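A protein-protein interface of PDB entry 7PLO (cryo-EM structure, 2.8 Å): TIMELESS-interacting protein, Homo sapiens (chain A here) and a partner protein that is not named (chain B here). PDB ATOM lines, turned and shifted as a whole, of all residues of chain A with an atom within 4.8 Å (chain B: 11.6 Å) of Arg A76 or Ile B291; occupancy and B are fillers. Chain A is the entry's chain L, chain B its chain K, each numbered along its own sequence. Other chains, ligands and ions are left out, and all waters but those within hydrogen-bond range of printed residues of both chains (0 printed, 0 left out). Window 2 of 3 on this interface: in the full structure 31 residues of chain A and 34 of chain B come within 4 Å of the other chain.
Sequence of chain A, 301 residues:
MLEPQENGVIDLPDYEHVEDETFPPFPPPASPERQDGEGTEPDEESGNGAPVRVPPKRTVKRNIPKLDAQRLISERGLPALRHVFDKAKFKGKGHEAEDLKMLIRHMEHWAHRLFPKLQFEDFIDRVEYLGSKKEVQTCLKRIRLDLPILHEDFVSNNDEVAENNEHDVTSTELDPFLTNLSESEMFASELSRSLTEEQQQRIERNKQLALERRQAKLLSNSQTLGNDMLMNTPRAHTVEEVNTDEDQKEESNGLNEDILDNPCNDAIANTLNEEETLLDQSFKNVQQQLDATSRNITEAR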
ATOM      1  N   LEU A  72      18.659  26.770   8.567  1.00  0.00           N
ATOM      2  CA  LEU A  72      17.860  25.610   8.951  1.00  0.00           C
ATOM      3  C   LEU A  72      16.434  25.601   8.415  1.00  0.00           C
ATOM      4  O   LEU A  72      15.836  24.519   8.373  1.00  0.00           O
ATOM      5  CB  LEU A  72      17.810  25.482  10.484  1.00  0.00           C
ATOM      6  CG  LEU A  72      17.006  26.450  11.365  1.00  0.00           C
ATOM      7  CD1 LEU A  72      17.239  26.069  12.814  1.00  0.00           C
ATOM      8  CD2 LEU A  72      17.338  27.908  11.163  1.00  0.00           C
ATOM      9  N   SER A  74      15.026  25.783   5.503  1.00  0.00           N
ATOM     10  CA  SER A  74      14.852  24.911   4.343  1.00  0.00           C
ATOM     11  C   SER A  74      15.714  23.652   4.407  1.00  0.00           C
ATOM     12  O   SER A  74      15.790  22.921   3.413  1.00  0.00           O
ATOM     13  CB  SER A  74      15.153  25.691   3.060  1.00  0.00           C
ATOM     14  OG  SER A  74      16.370  26.408   3.167  1.00  0.00           O
ATOM     15  N   GLU A  75      16.345  23.367   5.553  1.00  0.00           N
ATOM     16  CA  GLU A  75      17.250  22.231   5.710  1.00  0.00           C
ATOM     17  C   GLU A  75      16.698  21.206   6.694  1.00  0.00           C
ATOM     18  O   GLU A  75      16.544  20.034   6.341  1.00  0.00           O
ATOM     19  CB  GLU A  75      18.636  22.719   6.164  1.00  0.00           C
ATOM     20  CG  GLU A  75      19.434  23.499   5.108  1.00  0.00           C
ATOM     21  CD  GLU A  75      18.911  24.906   4.855  1.00  0.00           C
ATOM     22  OE1 GLU A  75      18.333  25.511   5.783  1.00  0.00           O
ATOM     23  OE2 GLU A  75      19.065  25.402   3.719  1.00  0.00           O
ATOM     24  N   ARG A  76      16.409  21.623   7.930  1.00  0.00           N
ATOM     25  CA  ARG A  76      15.661  20.829   8.897  1.00  0.00           C
ATOM     26  C   ARG A  76      14.232  21.326   9.080  1.00  0.00           C
ATOM     27  O   ARG A  76      13.491  20.755   9.889  1.00  0.00           O
ATOM     28  CB  ARG A  76      16.385  20.833  10.253  1.00  0.00           C
ATOM     29  CG  ARG A  76      16.105  19.620  11.137  1.00  0.00           C
ATOM     30  CD  ARG A  76      16.676  19.803  12.538  1.00  0.00           C
ATOM     31  NE  ARG A  76      17.219  18.561  13.079  1.00  0.00           N
ATOM     32  CZ  ARG A  76      17.564  18.362  14.347  1.00  0.00           C
ATOM     33  NH1 ARG A  76      17.397  19.296  15.273  1.00  0.00           N
ATOM     34  NH2 ARG A  76      18.088  17.191  14.697  1.00  0.00           N
ATOM     35  N   GLY A  77      13.814  22.351   8.337  1.00  0.00           N
ATOM     36  CA  GLY A  77      12.536  23.001   8.554  1.00  0.00           C
ATOM     37  C   GLY A  77      11.455  22.497   7.622  1.00  0.00           C
ATOM     38  O   GLY A  77      10.867  21.446   7.878  1.00  0.00           O
ATOM     39  N   LEU A  78      11.173  23.254   6.559  1.00  0.00           N
ATOM     40  CA  LEU A  78      10.101  22.888   5.633  1.00  0.00           C
ATOM     41  C   LEU A  78      10.223  21.490   5.026  1.00  0.00           C
ATOM     42  O   LEU A  78       9.176  20.832   4.872  1.00  0.00           O
ATOM     43  CB  LEU A  78      10.002  23.939   4.514  1.00  0.00           C
ATOM     44  CG  LEU A  78       9.333  25.306   4.761  1.00  0.00           C
ATOM     45  CD1 LEU A  78       7.947  25.193   5.399  1.00  0.00           C
ATOM     46  CD2 LEU A  78      10.222  26.229   5.582  1.00  0.00           C
ATOM     47  N   ALA A  80      11.272  18.760   6.412  1.00  0.00           N
ATOM     48  CA  ALA A  80      10.763  17.856   7.439  1.00  0.00           C
ATOM     49  C   ALA A  80       9.293  18.126   7.743  1.00  0.00           C
ATOM     50  O   ALA A  80       8.534  17.193   8.035  1.00  0.00           O
ATOM     51  CB  ALA A  80      11.601  17.986   8.710  1.00  0.00           C
ATOM     52  N   TRP A 110       7.965  20.329  15.955  1.00  0.00           N
ATOM     53  CA  TRP A 110       8.820  20.590  14.798  1.00  0.00           C
ATOM     54  C   TRP A 110       9.623  21.872  14.988  1.00  0.00           C
ATOM     55  O   TRP A 110      10.837  21.907  14.738  1.00  0.00           O
ATOM     56  CB  TRP A 110       7.966  20.672  13.532  1.00  0.00           C
ATOM     57  CG  TRP A 110       8.665  21.324  12.379  1.00  0.00           C
ATOM     58  CD1 TRP A 110       9.590  20.759  11.556  1.00  0.00           C
ATOM     59  CD2 TRP A 110       8.488  22.670  11.920  1.00  0.00           C
ATOM     60  NE1 TRP A 110      10.005  21.668  10.614  1.00  0.00           N
ATOM     61  CE2 TRP A 110       9.344  22.851  10.818  1.00  0.00           C
ATOM     62  CE3 TRP A 110       7.693  23.741  12.338  1.00  0.00           C
ATOM     63  CZ2 TRP A 110       9.425  24.055  10.125  1.00  0.00           C
ATOM     64  CZ3 TRP A 110       7.776  24.938  11.650  1.00  0.00           C
ATOM     65  CH2 TRP A 110       8.635  25.085  10.556  1.00  0.00           C
ATOM     66  N   HIS A 112      10.456  23.316  17.806  1.00  0.00           N
ATOM     67  CA  HIS A 112      11.447  23.142  18.862  1.00  0.00           C
ATOM     68  C   HIS A 112      12.679  22.424  18.342  1.00  0.00           C
ATOM     69  O   HIS A 112      13.812  22.854  18.586  1.00  0.00           O
ATOM     70  CB  HIS A 112      10.869  22.364  20.041  1.00  0.00           C
ATOM     71  CG  HIS A 112      11.887  22.053  21.093  1.00  0.00           C
ATOM     72  ND1 HIS A 112      12.042  20.799  21.644  1.00  0.00           N
ATOM     73  CD2 HIS A 112      12.829  22.835  21.670  1.00  0.00           C
ATOM     74  CE1 HIS A 112      13.024  20.829  22.529  1.00  0.00           C
ATOM     75  NE2 HIS A 112      13.516  22.054  22.565  1.00  0.00           N
ATOM     76  N   ARG A 113      12.478  21.314  17.626  1.00  0.00           N
ATOM     77  CA  ARG A 113      13.631  20.597  17.091  1.00  0.00           C
ATOM     78  C   ARG A 113      14.373  21.429  16.058  1.00  0.00           C
ATOM     79  O   ARG A 113      15.579  21.236  15.862  1.00  0.00           O
ATOM     80  CB  ARG A 113      13.203  19.268  16.481  1.00  0.00           C
ATOM     81  CG  ARG A 113      12.580  18.320  17.476  1.00  0.00           C
ATOM     82  CD  ARG A 113      12.406  16.930  16.895  1.00  0.00           C
ATOM     83  NE  ARG A 113      13.668  16.198  16.810  1.00  0.00           N
ATOM     84  CZ  ARG A 113      14.443  16.088  15.736  1.00  0.00           C
ATOM     85  NH1 ARG A 113      14.134  16.657  14.580  1.00  0.00           N
ATOM     86  NH2 ARG A 113      15.567  15.383  15.824  1.00  0.00           N
ATOM     87  N   LEU A 114      13.687  22.361  15.396  1.00  0.00           N
ATOM     88  CA  LEU A 114      14.373  23.223  14.447  1.00  0.00           C
ATOM     89  C   LEU A 114      15.240  24.248  15.169  1.00  0.00           C
ATOM     90  O   LEU A 114      16.471  24.156  15.111  1.00  0.00           O
ATOM     91  CB  LEU A 114      13.352  23.916  13.542  1.00  0.00           C
ATOM     92  CG  LEU A 114      13.894  24.778  12.403  1.00  0.00           C
ATOM     93  CD1 LEU A 114      14.676  23.927  11.431  1.00  0.00           C
ATOM     94  CD2 LEU A 114      12.759  25.486  11.693  1.00  0.00           C
ATOM     95  N   PRO A 116      15.701  25.503  18.975  1.00  0.00           N
ATOM     96  CA  PRO A 116      15.229  25.280  20.346  1.00  0.00           C
ATOM     97  C   PRO A 116      15.380  26.478  21.271  1.00  0.00           C
ATOM     98  O   PRO A 116      14.987  26.384  22.439  1.00  0.00           O
ATOM     99  CB  PRO A 116      16.114  24.119  20.812  1.00  0.00           C
ATOM    100  CG  PRO A 116      17.405  24.394  20.162  1.00  0.00           C
ATOM    101  CD  PRO A 116      17.078  24.985  18.816  1.00  0.00           C
ATOM    102  N   VAL B 285       9.796   9.688  27.046  1.00  0.00           N
ATOM    103  CA  VAL B 285       8.647   9.751  26.147  1.00  0.00           C
ATOM    104  C   VAL B 285       9.140   9.175  24.824  1.00  0.00           C
ATOM    105  O   VAL B 285       9.813   9.856  24.049  1.00  0.00           O
ATOM    106  CB  VAL B 285       8.104  11.176  25.996  1.00  0.00           C
ATOM    107  CG1 VAL B 285       6.871  11.179  25.066  1.00  0.00           C
ATOM    108  CG2 VAL B 285       7.790  11.822  27.384  1.00  0.00           C
ATOM    109  N   GLN B 286       8.811   7.904  24.577  1.00  0.00           N
ATOM    110  CA  GLN B 286       9.493   7.133  23.540  1.00  0.00           C
ATOM    111  C   GLN B 286       9.231   7.691  22.145  1.00  0.00           C
ATOM    112  O   GLN B 286      10.130   7.697  21.296  1.00  0.00           O
ATOM    113  CB  GLN B 286       9.066   5.668  23.618  1.00  0.00           C
ATOM    114  CG  GLN B 286       9.500   4.971  24.899  1.00  0.00           C
ATOM    115  CD  GLN B 286       9.196   3.486  24.892  1.00  0.00           C
ATOM    116  OE1 GLN B 286      10.083   2.660  25.103  1.00  0.00           O
ATOM    117  NE2 GLN B 286       7.937   3.139  24.654  1.00  0.00           N
ATOM    118  N   GLY B 287       8.010   8.161  21.885  1.00  0.00           N
ATOM    119  CA  GLY B 287       7.694   8.659  20.559  1.00  0.00           C
ATOM    120  C   GLY B 287       8.359   9.981  20.230  1.00  0.00           C
ATOM    121  O   GLY B 287       8.689  10.236  19.068  1.00  0.00           O
ATOM    122  N   LEU B 288       8.571  10.831  21.232  1.00  0.00           N
ATOM    123  CA  LEU B 288       9.088  12.178  21.001  1.00  0.00           C
ATOM    124  C   LEU B 288      10.602  12.130  20.866  1.00  0.00           C
ATOM    125  O   LEU B 288      11.311  11.815  21.828  1.00  0.00           O
ATOM    126  CB  LEU B 288       8.685  13.114  22.138  1.00  0.00           C
ATOM    127  CG  LEU B 288       7.231  13.579  22.243  1.00  0.00           C
ATOM    128  CD1 LEU B 288       7.065  14.430  23.490  1.00  0.00           C
ATOM    129  CD2 LEU B 288       6.789  14.360  21.013  1.00  0.00           C
ATOM    130  N   LYS B 289      11.100  12.448  19.676  1.00  0.00           N
ATOM    131  CA  LYS B 289      12.527  12.668  19.503  1.00  0.00           C
ATOM    132  C   LYS B 289      12.921  13.991  20.144  1.00  0.00           C
ATOM    133  O   LYS B 289      12.181  14.976  20.081  1.00  0.00           O
ATOM    134  CB  LYS B 289      12.894  12.668  18.019  1.00  0.00           C
ATOM    135  CG  LYS B 289      12.578  11.361  17.300  1.00  0.00           C
ATOM    136  CD  LYS B 289      12.929  11.414  15.817  1.00  0.00           C
ATOM    137  CE  LYS B 289      14.433  11.375  15.580  1.00  0.00           C
ATOM    138  NZ  LYS B 289      14.763  11.169  14.142  1.00  0.00           N
ATOM    139  N   SER B 290      14.096  14.011  20.764  1.00  0.00           N
ATOM    140  CA  SER B 290      14.615  15.215  21.395  1.00  0.00           C
ATOM    141  C   SER B 290      15.181  16.130  20.310  1.00  0.00           C
ATOM    142  O   SER B 290      14.932  15.936  19.116  1.00  0.00           O
ATOM    143  CB  SER B 290      15.651  14.840  22.449  1.00  0.00           C
ATOM    144  OG  SER B 290      16.768  14.203  21.856  1.00  0.00           O
ATOM    145  N   ILE B 291      15.937  17.159  20.701  1.00  0.00           N
ATOM    146  CA  ILE B 291      16.596  17.987  19.694  1.00  0.00           C
ATOM    147  C   ILE B 291      17.641  17.172  18.938  1.00  0.00           C
ATOM    148  O   ILE B 291      17.948  17.466  17.776  1.00  0.00           O
ATOM    149  CB  ILE B 291      17.191  19.268  20.326  1.00  0.00           C
ATOM    150  CG1 ILE B 291      18.233  18.968  21.413  1.00  0.00           C
ATOM    151  CG2 ILE B 291      16.064  20.122  20.908  1.00  0.00           C
ATOM    152  CD1 ILE B 291      19.066  20.181  21.797  1.00  0.00           C
ATOM    153  N   GLY B 292      18.204  16.148  19.579  1.00  0.00           N
ATOM    154  CA  GLY B 292      18.947  15.108  18.896  1.00  0.00           C
ATOM    155  C   GLY B 292      18.016  14.016  18.411  1.00  0.00           C
ATOM    156  O   GLY B 292      16.808  14.215  18.263  1.00  0.00           O
ATOM    157  N   GLU B 293      18.593  12.840  18.161  1.00  0.00           N
ATOM    158  CA  GLU B 293      17.813  11.681  17.738  1.00  0.00           C
ATOM    159  C   GLU B 293      17.299  10.839  18.904  1.00  0.00           C
ATOM    160  O   GLU B 293      16.456   9.962  18.685  1.00  0.00           O
ATOM    161  CB  GLU B 293      18.634  10.799  16.770  1.00  0.00           C
ATOM    162  CG  GLU B 293      19.803   9.961  17.344  1.00  0.00           C
ATOM    163  CD  GLU B 293      21.062  10.767  17.598  1.00  0.00           C
ATOM    164  OE1 GLU B 293      20.965  12.003  17.734  1.00  0.00           O
ATOM    165  OE2 GLU B 293      22.153  10.160  17.658  1.00  0.00           O
ATOM    166  N   ARG B 294      17.781  11.074  20.122  1.00  0.00           N
ATOM    167  CA  ARG B 294      17.382  10.275  21.270  1.00  0.00           C
ATOM    168  C   ARG B 294      15.997  10.689  21.760  1.00  0.00           C
ATOM    169  O   ARG B 294      15.537  11.812  21.534  1.00  0.00           O
ATOM    170  CB  ARG B 294      18.407  10.416  22.398  1.00  0.00           C
ATOM    171  CG  ARG B 294      19.812   9.964  22.012  1.00  0.00           C
ATOM    172  CD  ARG B 294      20.828  10.214  23.115  1.00  0.00           C
ATOM    173  NE  ARG B 294      20.599   9.385  24.294  1.00  0.00           N
ATOM    174  CZ  ARG B 294      20.883   8.091  24.387  1.00  0.00           C
ATOM    175  NH1 ARG B 294      21.360   7.404  23.359  1.00  0.00           N
ATOM    176  NH2 ARG B 294      20.682   7.466  25.543  1.00  0.00           N
ATOM    177  N   ASP B 295      15.328   9.758  22.434  1.00  0.00           N
ATOM    178  CA  ASP B 295      14.002  10.026  22.970  1.00  0.00           C
ATOM    179  C   ASP B 295      14.065  11.094  24.057  1.00  0.00           C
ATOM    180  O   ASP B 295      15.065  11.235  24.766  1.00  0.00           O
ATOM    181  CB  ASP B 295      13.383   8.749  23.539  1.00  0.00           C
ATOM    182  CG  ASP B 295      13.225   7.662  22.496  1.00  0.00           C
ATOM    183  OD1 ASP B 295      13.479   7.937  21.305  1.00  0.00           O
ATOM    184  OD2 ASP B 295      12.849   6.530  22.868  1.00  0.00           O
ATOM    185  N   LEU B 296      12.979  11.852  24.179  1.00  0.00           N
ATOM    186  CA  LEU B 296      12.908  12.915  25.171  1.00  0.00           C
ATOM    187  C   LEU B 296      12.899  12.329  26.575  1.00  0.00           C
ATOM    188  O   LEU B 296      12.130  11.409  26.869  1.00  0.00           O
ATOM    189  CB  LEU B 296      11.651  13.758  24.944  1.00  0.00           C
ATOM    190  CG  LEU B 296      11.404  14.973  25.849  1.00  0.00           C
ATOM    191  CD1 LEU B 296      12.361  16.101  25.512  1.00  0.00           C
ATOM    192  CD2 LEU B 296       9.961  15.436  25.737  1.00  0.00           C
ATOM    193  N   ILE B 297      13.754  12.868  27.442  1.00  0.00           N
ATOM    194  CA  ILE B 297      13.729  12.585  28.874  1.00  0.00           C
ATOM    195  C   ILE B 297      13.013  13.753  29.537  1.00  0.00           C
ATOM    196  O   ILE B 297      13.436  14.907  29.400  1.00  0.00           O
ATOM    197  CB  ILE B 297      15.144  12.385  29.454  1.00  0.00           C
ATOM    198  CG1 ILE B 297      15.896  11.272  28.699  1.00  0.00           C
ATOM    199  CG2 ILE B 297      15.073  12.025  30.963  1.00  0.00           C
ATOM    200  CD1 ILE B 297      17.361  11.101  29.090  1.00  0.00           C
ATOM    201  N   PHE B 298      11.936  13.451  30.258  1.00  0.00           N
ATOM    202  CA  PHE B 298      11.102  14.444  30.918  1.00  0.00           C
ATOM    203  C   PHE B 298      11.336  14.385  32.421  1.00  0.00           C
ATOM    204  O   PHE B 298      11.275  13.300  33.023  1.00  0.00           O
ATOM    205  CB  PHE B 298       9.624  14.210  30.603  1.00  0.00           C
ATOM    206  CG  PHE B 298       8.759  15.400  30.874  1.00  0.00           C
ATOM    207  CD1 PHE B 298       8.688  16.439  29.964  1.00  0.00           C
ATOM    208  CD2 PHE B 298       8.015  15.486  32.036  1.00  0.00           C
ATOM    209  CE1 PHE B 298       7.897  17.538  30.210  1.00  0.00           C
ATOM    210  CE2 PHE B 298       7.223  16.587  32.283  1.00  0.00           C
ATOM    211  CZ  PHE B 298       7.158  17.607  31.364  1.00  0.00           C
ATOM    212  N   TYR B 308       1.691  18.696  28.098  1.00  0.00           N
ATOM    213  CA  TYR B 308       3.073  18.913  27.679  1.00  0.00           C
ATOM    214  C   TYR B 308       3.201  19.987  26.605  1.00  0.00           C
ATOM    215  O   TYR B 308       2.409  20.052  25.662  1.00  0.00           O
ATOM    216  CB  TYR B 308       3.664  17.608  27.138  1.00  0.00           C
ATOM    217  CG  TYR B 308       5.039  17.779  26.540  1.00  0.00           C
ATOM    218  CD1 TYR B 308       6.142  17.973  27.351  1.00  0.00           C
ATOM    219  CD2 TYR B 308       5.233  17.760  25.165  1.00  0.00           C
ATOM    220  CE1 TYR B 308       7.402  18.138  26.820  1.00  0.00           C
ATOM    221  CE2 TYR B 308       6.491  17.926  24.621  1.00  0.00           C
ATOM    222  CZ  TYR B 308       7.572  18.114  25.453  1.00  0.00           C
ATOM    223  OH  TYR B 308       8.829  18.279  24.923  1.00  0.00           O
ATOM    224  N   SER B 309       4.218  20.832  26.766  1.00  0.00           N
ATOM    225  CA  SER B 309       4.701  21.704  25.707  1.00  0.00           C
ATOM    226  C   SER B 309       6.194  21.907  25.916  1.00  0.00           C
ATOM    227  O   SER B 309       6.679  21.917  27.050  1.00  0.00           O
ATOM    228  CB  SER B 309       3.968  23.049  25.692  1.00  0.00           C
ATOM    229  OG  SER B 309       4.171  23.754  26.902  1.00  0.00           O
ATOM    230  N   SER B 310       6.923  22.066  24.809  1.00  0.00           N
ATOM    231  CA  SER B 310       8.375  22.195  24.880  1.00  0.00           C
ATOM    232  C   SER B 310       8.831  23.500  25.529  1.00  0.00           C
ATOM    233  O   SER B 310      10.002  23.598  25.911  1.00  0.00           O
ATOM    234  CB  SER B 310       8.977  22.087  23.478  1.00  0.00           C
ATOM    235  OG  SER B 310       8.708  20.819  22.906  1.00  0.00           O
ATOM    236  N   ASP B 311       7.947  24.492  25.662  1.00  0.00           N
ATOM    237  CA  ASP B 311       8.286  25.791  26.237  1.00  0.00           C
ATOM    238  C   ASP B 311       7.916  25.888  27.716  1.00  0.00           C
ATOM    239  O   ASP B 311       7.652  26.984  28.220  1.00  0.00           O
ATOM    240  CB  ASP B 311       7.622  26.919  25.440  1.00  0.00           C
ATOM    241  CG  ASP B 311       6.104  26.795  25.372  1.00  0.00           C
ATOM    242  OD1 ASP B 311       5.546  25.831  25.938  1.00  0.00           O
ATOM    243  OD2 ASP B 311       5.470  27.661  24.735  1.00  0.00           O
ATOM    244  N   LYS B 314      11.267  27.539  29.301  1.00  0.00           N
ATOM    245  CA  LYS B 314      12.012  28.508  28.508  1.00  0.00           C
ATOM    246  C   LYS B 314      11.768  29.928  28.998  1.00  0.00           C
ATOM    247  O   LYS B 314      10.648  30.290  29.367  1.00  0.00           O
ATOM    248  CB  LYS B 314      11.619  28.410  27.036  1.00  0.00           C
ATOM    249  CG  LYS B 314      12.084  27.150  26.348  1.00  0.00           C
ATOM    250  CD  LYS B 314      11.695  27.182  24.889  1.00  0.00           C
ATOM    251  CE  LYS B 314      12.121  25.930  24.163  1.00  0.00           C
ATOM    252  NZ  LYS B 314      11.645  25.969  22.760  1.00  0.00           N
ATOM    253  N   VAL B 790       2.017  23.257   5.547  1.00  0.00           N
ATOM    254  CA  VAL B 790       3.085  24.191   5.203  1.00  0.00           C
ATOM    255  C   VAL B 790       2.503  25.568   4.906  1.00  0.00           C
ATOM    256  O   VAL B 790       3.107  26.594   5.242  1.00  0.00           O
ATOM    257  CB  VAL B 790       3.916  23.658   4.020  1.00  0.00           C
ATOM    258  CG1 VAL B 790       4.871  24.744   3.490  1.00  0.00           C
ATOM    259  CG2 VAL B 790       4.685  22.393   4.427  1.00  0.00           C
ATOM    260  N   LEU B 793       2.178  28.390   7.618  1.00  0.00           N
ATOM    261  CA  LEU B 793       3.341  28.984   8.265  1.00  0.00           C
ATOM    262  C   LEU B 793       3.597  30.440   7.877  1.00  0.00           C
ATOM    263  O   LEU B 793       4.339  31.118   8.597  1.00  0.00           O
ATOM    264  CB  LEU B 793       4.575  28.133   7.943  1.00  0.00           C
ATOM    265  CG  LEU B 793       5.858  28.296   8.766  1.00  0.00           C
ATOM    266  CD1 LEU B 793       5.644  27.960  10.233  1.00  0.00           C
ATOM    267  CD2 LEU B 793       6.952  27.408   8.190  1.00  0.00           C
ATOM    268  N   PHE B 794       3.011  30.939   6.780  1.00  0.00           N
ATOM    269  CA  PHE B 794       3.327  32.269   6.260  1.00  0.00           C
ATOM    270  C   PHE B 794       2.065  33.009   5.830  1.00  0.00           C
ATOM    271  O   PHE B 794       1.061  32.397   5.454  1.00  0.00           O
ATOM    272  CB  PHE B 794       4.275  32.198   5.054  1.00  0.00           C
ATOM    273  CG  PHE B 794       5.511  31.383   5.296  1.00  0.00           C
ATOM    274  CD1 PHE B 794       6.516  31.853   6.122  1.00  0.00           C
ATOM    275  CD2 PHE B 794       5.674  30.153   4.684  1.00  0.00           C
ATOM    276  CE1 PHE B 794       7.655  31.108   6.340  1.00  0.00           C
ATOM    277  CE2 PHE B 794       6.812  29.405   4.899  1.00  0.00           C
ATOM    278  CZ  PHE B 794       7.803  29.884   5.728  1.00  0.00           C
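The guanidinium group (NE) of Arg A113 is in hydrogen-bond range of the backbone carbonyl oxygen (O) of Ser B290 (2.6 Å). O of Ile B291 sits at hydrogen-bond distance from NH2 of Arg A76 (3.1 Å). The backbone carbonyl oxygen (O) of Gly B292 sits at hydrogen-bond distance from the guanidinium group (NH2) of Arg A113. The side-chain amino group (NZ) of Lys B314 sits close to the backbone carbonyl oxygen (O) of Pro A116, 3.4 Å away.
OG of Ser B290 sits close to N of Gly B292 (3.3 Å). The side-chain hydroxyl (OG) of Ser B290 sits at hydrogen-bond distance from the backbone carbonyl oxygen (O) of Arg B294. OH of Tyr B308 is in hydrogen-bond range of OG of Ser B310, at 3.2 Å. The guanidinium group (NH1) of Arg A76 is in hydrogen-bond range of the backbone carbonyl oxygen (O) of Arg A113 (2.7 Å). The indole nitrogen of Trp A110 sits at hydrogen-bond distance from the backbone carbonyl oxygen of Gly A77, at 2.9 Å.
Val B790 touches Leu A78 (CG1 to CD1, 3.6 Å). CD1 of Leu A78 touches CD2 of Leu B793 (3.7 Å). Trp A110 touches Leu B793 (CH2 to CD2, 3.7 Å). CG2 of Ile B291 touches CE1 of His A112, at 3.5 Å. Ser B310 touches His A112 (OG to ND1, 3.6 Å). CD2 of His A112 touches NZ of Lys B314 (3.5 Å). Arg A113 touches Lys B289 (CD to O, 3.7 Å). O of Ile B291 touches NH2 of Arg A113 (3.7 Å). Ile B291 touches Pro A116.
No residue of chain B comes within 4 Å of Ser A74. No residue of chain B comes within 4 Å of Glu A75. Arg A76 touches one residue of chain B. No residue of chain B comes within 4 Å of Gly A77. Of the printed residues of chain B, Trp A110 touches Leu B793. His A112 touches just these residues of chain B: Ile B291 (3.5 Å), Ser B310 (3.6 Å) and Lys B314 (3.5 Å). Of the printed residues of chain B, Pro A116 touches Ile B291 and Lys B314. Gly B287 touches none of the printed residues of chain A. Of the printed residues of chain A, Ser B290 touches Arg A113 (2.6 Å). Printed residues of chain A within 4 Å of Ile B291: Arg A76, His A112, Arg A113 and Pro A116. Asp B311 touches none of the printed residues of chain A. The nearest residue of chain B that does not touch Arg A76 is Gly B292 (4.8 Å). The nearest printed residue of chain A that does not touch Lys B289 is His A112 (6.0 Å).
Of the 22 printed residues of chain B, 8 touch a printed residue of chain A. Hydrophobic or aromatic side chains of chain B within 4 Å of the printed part of chain A: Ile B291, Val B790 and Leu B793. Of the 12 printed residues of chain A, 6 touch a printed residue of chain B. Hydrophobic or aromatic side chains of chain A that line the printed part of chain B: Leu A78, Trp A110, His A112 and Pro A116. Along chain A the printed residues that touch a printed residue of chain B span positions 76 to 116. Among the printed residues, 13 pairs touch across the chains. Among the printed residues, no Asp or Glu carboxylate lies within 4 Å of a Lys or Arg side-chain nitrogen of the other chain.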
